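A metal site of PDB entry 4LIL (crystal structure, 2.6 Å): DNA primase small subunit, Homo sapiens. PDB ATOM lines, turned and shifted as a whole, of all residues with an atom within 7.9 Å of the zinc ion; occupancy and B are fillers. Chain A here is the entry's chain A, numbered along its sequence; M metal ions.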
ATOM      1  N   MET A 116     -31.417 -13.374  28.398  1.00  0.00           N
ATOM      2  CA  MET A 116     -31.225 -14.659  27.715  1.00  0.00           C
ATOM      3  C   MET A 116     -32.269 -14.968  26.616  1.00  0.00           C
ATOM      4  O   MET A 116     -31.965 -15.650  25.650  1.00  0.00           O
ATOM      5  CB  MET A 116     -31.167 -15.802  28.736  1.00  0.00           C
ATOM      6  CG  MET A 116     -30.628 -17.109  28.206  1.00  0.00           C
ATOM      7  SD  MET A 116     -28.827 -17.183  28.214  1.00  0.00           S
ATOM      8  CE  MET A 116     -28.598 -16.980  29.956  1.00  0.00           C
ATOM      9  N   ARG A 123     -30.726 -21.237  21.209  1.00  0.00           N
ATOM     10  CA  ARG A 123     -30.644 -22.288  22.222  1.00  0.00           C
ATOM     11  C   ARG A 123     -31.483 -23.521  21.910  1.00  0.00           C
ATOM     12  O   ARG A 123     -32.568 -23.405  21.335  1.00  0.00           O
ATOM     13  CB  ARG A 123     -31.091 -21.736  23.567  1.00  0.00           C
ATOM     14  CG  ARG A 123     -30.234 -20.634  24.101  1.00  0.00           C
ATOM     15  CD  ARG A 123     -30.683 -20.303  25.479  1.00  0.00           C
ATOM     16  NE  ARG A 123     -32.043 -19.763  25.490  1.00  0.00           N
ATOM     17  CZ  ARG A 123     -32.730 -19.531  26.603  1.00  0.00           C
ATOM     18  NH1 ARG A 123     -32.203 -19.826  27.779  1.00  0.00           N
ATOM     19  NH2 ARG A 123     -33.966 -19.028  26.550  1.00  0.00           N
ATOM     20  N   ARG A 124     -30.999 -24.702  22.300  1.00  0.00           N
ATOM     21  CA  ARG A 124     -31.727 -25.968  22.098  1.00  0.00           C
ATOM     22  C   ARG A 124     -32.241 -26.553  23.404  1.00  0.00           C
ATOM     23  O   ARG A 124     -32.734 -27.686  23.432  1.00  0.00           O
ATOM     24  CB  ARG A 124     -30.835 -27.002  21.391  1.00  0.00           C
ATOM     25  CG  ARG A 124     -30.645 -26.773  19.903  1.00  0.00           C
ATOM     26  CD  ARG A 124     -29.540 -27.650  19.328  1.00  0.00           C
ATOM     27  NE  ARG A 124     -29.943 -29.038  19.093  1.00  0.00           N
ATOM     28  CZ  ARG A 124     -29.659 -30.055  19.909  1.00  0.00           C
ATOM     29  NH1 ARG A 124     -28.963 -29.838  21.017  1.00  0.00           N
ATOM     30  NH2 ARG A 124     -30.081 -31.284  19.615  1.00  0.00           N
ATOM     31  N   CYS A 125     -32.140 -25.787  24.473  1.00  0.00           N
ATOM     32  CA  CYS A 125     -32.370 -26.291  25.811  1.00  0.00           C
ATOM     33  C   CYS A 125     -33.377 -25.470  26.616  1.00  0.00           C
ATOM     34  O   CYS A 125     -34.031 -26.005  27.510  1.00  0.00           O
ATOM     35  CB  CYS A 125     -31.041 -26.318  26.579  1.00  0.00           C
ATOM     36  SG  CYS A 125     -30.158 -24.737  26.581  1.00  0.00           S
ATOM     37  N   CYS A 126     -33.503 -24.192  26.314  1.00  0.00           N
ATOM     38  CA  CYS A 126     -34.289 -23.308  27.183  1.00  0.00           C
ATOM     39  C   CYS A 126     -35.106 -22.204  26.488  1.00  0.00           C
ATOM     40  O   CYS A 126     -34.690 -21.631  25.476  1.00  0.00           O
ATOM     41  CB  CYS A 126     -33.384 -22.685  28.268  1.00  0.00           C
ATOM     42  SG  CYS A 126     -32.844 -23.846  29.578  1.00  0.00           S
ATOM     43  N   SER A 127     -36.243 -21.890  27.097  1.00  0.00           N
ATOM     44  CA  SER A 127     -37.186 -20.926  26.545  1.00  0.00           C
ATOM     45  C   SER A 127     -37.829 -20.046  27.619  1.00  0.00           C
ATOM     46  O   SER A 127     -37.184 -19.159  28.178  1.00  0.00           O
ATOM     47  CB  SER A 127     -38.268 -21.661  25.746  1.00  0.00           C
ATOM     48  OG  SER A 127     -38.773 -22.770  26.485  1.00  0.00           O
ATOM     49  N   ASP A 130     -36.212 -18.952  31.438  1.00  0.00           N
ATOM     50  CA  ASP A 130     -35.455 -20.171  31.694  1.00  0.00           C
ATOM     51  C   ASP A 130     -33.986 -20.072  31.296  1.00  0.00           C
ATOM     52  O   ASP A 130     -33.629 -19.377  30.340  1.00  0.00           O
ATOM     53  CB  ASP A 130     -36.095 -21.380  31.004  1.00  0.00           C
ATOM     54  CG  ASP A 130     -37.146 -22.064  31.868  1.00  0.00           C
ATOM     55  OD1 ASP A 130     -37.217 -21.760  33.082  1.00  0.00           O
ATOM     56  OD2 ASP A 130     -37.904 -22.897  31.343  1.00  0.00           O
ATOM     57  N   ILE A 131     -33.143 -20.761  32.069  1.00  0.00           N
ATOM     58  CA  ILE A 131     -31.697 -20.832  31.846  1.00  0.00           C
ATOM     59  C   ILE A 131     -31.220 -22.182  32.377  1.00  0.00           C
ATOM     60  O   ILE A 131     -32.001 -22.936  32.956  1.00  0.00           O
ATOM     61  CB  ILE A 131     -30.920 -19.770  32.630  1.00  0.00           C
ATOM     62  CG1 ILE A 131     -31.186 -19.914  34.126  1.00  0.00           C
ATOM     63  CG2 ILE A 131     -31.221 -18.347  32.116  1.00  0.00           C
ATOM     64  CD1 ILE A 131     -30.294 -18.988  34.955  1.00  0.00           C
ATOM     65  N   CYS A 132     -29.920 -22.455  32.194  1.00  0.00           N
ATOM     66  CA  CYS A 132     -29.296 -23.689  32.679  1.00  0.00           C
ATOM     67  C   CYS A 132     -27.789 -23.600  32.372  1.00  0.00           C
ATOM     68  O   CYS A 132     -27.345 -22.651  31.717  1.00  0.00           O
ATOM     69  CB  CYS A 132     -29.930 -24.902  32.013  1.00  0.00           C
ATOM     70  SG  CYS A 132     -29.491 -25.126  30.292  1.00  0.00           S
ATOM     71  N   PRO A 133     -26.989 -24.552  32.891  1.00  0.00           N
ATOM     72  CA  PRO A 133     -25.543 -24.520  32.633  1.00  0.00           C
ATOM     73  C   PRO A 133     -25.161 -24.459  31.170  1.00  0.00           C
ATOM     74  O   PRO A 133     -24.179 -23.783  30.794  1.00  0.00           O
ATOM     75  CB  PRO A 133     -25.077 -25.847  33.231  1.00  0.00           C
ATOM     76  CG  PRO A 133     -25.972 -25.994  34.431  1.00  0.00           C
ATOM     77  CD  PRO A 133     -27.318 -25.451  34.024  1.00  0.00           C
ATOM     78  N   LYS A 134     -25.949 -25.137  30.337  1.00  0.00           N
ATOM     79  CA  LYS A 134     -25.627 -25.329  28.934  1.00  0.00           C
ATOM     80  C   LYS A 134     -25.756 -24.057  28.076  1.00  0.00           C
ATOM     81  O   LYS A 134     -25.280 -24.028  26.942  1.00  0.00           O
ATOM     82  CB  LYS A 134     -26.481 -26.459  28.369  1.00  0.00           C
ATOM     83  CG  LYS A 134     -26.469 -27.723  29.237  1.00  0.00           C
ATOM     84  CD  LYS A 134     -27.162 -28.923  28.567  1.00  0.00           C
ATOM     85  CE  LYS A 134     -28.680 -28.774  28.582  1.00  0.00           C
ATOM     86  NZ  LYS A 134     -29.390 -30.064  28.500  1.00  0.00           N
ATOM     87  N   CYS A 135     -26.374 -22.992  28.596  1.00  0.00           N
ATOM     88  CA  CYS A 135     -26.637 -21.802  27.790  1.00  0.00           C
ATOM     89  C   CYS A 135     -26.266 -20.484  28.462  1.00  0.00           C
ATOM     90  O   CYS A 135     -26.410 -19.419  27.861  1.00  0.00           O
ATOM     91  CB  CYS A 135     -28.119 -21.759  27.403  1.00  0.00           C
ATOM     92  SG  CYS A 135     -29.262 -21.425  28.823  1.00  0.00           S
ATOM     93  N   TRP A 136     -25.790 -20.545  29.711  1.00  0.00           N
ATOM     94  CA  TRP A 136     -25.292 -19.382  30.448  1.00  0.00           C
ATOM     95  C   TRP A 136     -23.961 -18.850  29.884  1.00  0.00           C
ATOM     96  O   TRP A 136     -23.577 -17.651  30.050  1.00  0.00           O
ATOM     97  CB  TRP A 136     -25.114 -19.722  31.941  1.00  0.00           C
ATOM     98  CG  TRP A 136     -24.608 -18.526  32.706  1.00  0.00           C
ATOM     99  CD1 TRP A 136     -23.332 -18.326  33.146  1.00  0.00           C
ATOM    100  CD2 TRP A 136     -25.354 -17.367  33.079  1.00  0.00           C
ATOM    101  NE1 TRP A 136     -23.240 -17.108  33.772  1.00  0.00           N
ATOM    102  CE2 TRP A 136     -24.469 -16.493  33.735  1.00  0.00           C
ATOM    103  CE3 TRP A 136     -26.696 -16.988  32.910  1.00  0.00           C
ATOM    104  CZ2 TRP A 136     -24.879 -15.246  34.256  1.00  0.00           C
ATOM    105  CZ3 TRP A 136     -27.106 -15.749  33.412  1.00  0.00           C
ATOM    106  CH2 TRP A 136     -26.188 -14.898  34.077  1.00  0.00           C
ATOM    107  N   LEU A 138     -23.476 -18.132  27.009  1.00  0.00           N
ATOM    108  CA  LEU A 138     -23.867 -16.996  26.198  1.00  0.00           C
ATOM    109  C   LEU A 138     -23.613 -15.698  26.970  1.00  0.00           C
ATOM    110  O   LEU A 138     -23.069 -14.731  26.424  1.00  0.00           O
ATOM    111  CB  LEU A 138     -25.320 -17.114  25.793  1.00  0.00           C
ATOM    112  CG  LEU A 138     -25.508 -18.107  24.664  1.00  0.00           C
ATOM    113  CD1 LEU A 138     -26.987 -18.318  24.346  1.00  0.00           C
ATOM    114  CD2 LEU A 138     -24.759 -17.613  23.435  1.00  0.00           C
ATOM    115  N   TYR A 230     -19.235 -24.816  23.912  1.00  0.00           N
ATOM    116  CA  TYR A 230     -20.606 -24.309  23.994  1.00  0.00           C
ATOM    117  C   TYR A 230     -21.503 -24.788  22.845  1.00  0.00           C
ATOM    118  O   TYR A 230     -22.642 -25.171  23.041  1.00  0.00           O
ATOM    119  CB  TYR A 230     -20.642 -22.770  24.065  1.00  0.00           C
ATOM    120  CG  TYR A 230     -22.035 -22.234  23.751  1.00  0.00           C
ATOM    121  CD1 TYR A 230     -23.098 -22.460  24.619  1.00  0.00           C
ATOM    122  CD2 TYR A 230     -22.297 -21.550  22.568  1.00  0.00           C
ATOM    123  CE1 TYR A 230     -24.389 -22.016  24.332  1.00  0.00           C
ATOM    124  CE2 TYR A 230     -23.575 -21.105  22.268  1.00  0.00           C
ATOM    125  CZ  TYR A 230     -24.610 -21.338  23.150  1.00  0.00           C
ATOM    126  OH  TYR A 230     -25.879 -20.900  22.842  1.00  0.00           O
ATOM    127  N   GLN A 235     -24.464 -27.366  22.948  1.00  0.00           N
ATOM    128  CA  GLN A 235     -25.638 -27.181  22.104  1.00  0.00           C
ATOM    129  C   GLN A 235     -25.705 -28.178  20.951  1.00  0.00           C
ATOM    130  O   GLN A 235     -26.813 -28.532  20.520  1.00  0.00           O
ATOM    131  CB  GLN A 235     -25.685 -25.750  21.567  1.00  0.00           C
ATOM    132  CG  GLN A 235     -25.712 -24.689  22.640  1.00  0.00           C
ATOM    133  CD  GLN A 235     -26.815 -24.902  23.679  1.00  0.00           C
ATOM    134  OE1 GLN A 235     -28.007 -24.894  23.363  1.00  0.00           O
ATOM    135  NE2 GLN A 235     -26.403 -25.078  24.926  1.00  0.00           N
ATOM    136  N   PHE A 349     -26.926 -20.261  39.488  1.00  0.00           N
ATOM    137  CA  PHE A 349     -27.648 -21.197  40.321  1.00  0.00           C
ATOM    138  C   PHE A 349     -27.144 -21.232  41.755  1.00  0.00           C
ATOM    139  O   PHE A 349     -27.884 -21.650  42.644  1.00  0.00           O
ATOM    140  CB  PHE A 349     -27.638 -22.596  39.706  1.00  0.00           C
ATOM    141  CG  PHE A 349     -28.404 -22.661  38.424  1.00  0.00           C
ATOM    142  CD1 PHE A 349     -27.781 -22.356  37.206  1.00  0.00           C
ATOM    143  CD2 PHE A 349     -29.747 -22.999  38.420  1.00  0.00           C
ATOM    144  CE1 PHE A 349     -28.493 -22.417  36.008  1.00  0.00           C
ATOM    145  CE2 PHE A 349     -30.468 -23.053  37.230  1.00  0.00           C
ATOM    146  CZ  PHE A 349     -29.829 -22.759  36.027  1.00  0.00           C
HETATM  147 ZN    ZN M   1     -30.288 -23.571  28.793  1.00  0.00          ZN
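The guanidinium group (NH1) of Arg 123 lies close to the side-chain sulfur (SG) of Cys 135, at 3.5 Å.
SG of Cys 126 lies close to O of Ile 131 (3.6 Å).
NH2 of Arg 123 sits at hydrogen-bond distance from O of Cys 126, 2.9 Å away.
The side-chain sulfur of Cys 132 lies close to the backbone NH of Lys 134, 3.5 Å away.
C of Ile 131 touches the zinc ion (3.96 Å).
Within 4 Å of the zinc ion: Cys 125, Cys 126, Ile 131, Cys 132 and Cys 135.
Along chain A the residues within 4 Å of the zinc ion span positions 125 to 135.
The zinc ion is bound by the side-chain sulfur of Cys 132 (2.3 Å), the side-chain sulfur of Cys 135 (2.4 Å), the side-chain sulfur of Cys 125 (2.5 Å) and the side-chain sulfur of Cys 126 (2.7 Å).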
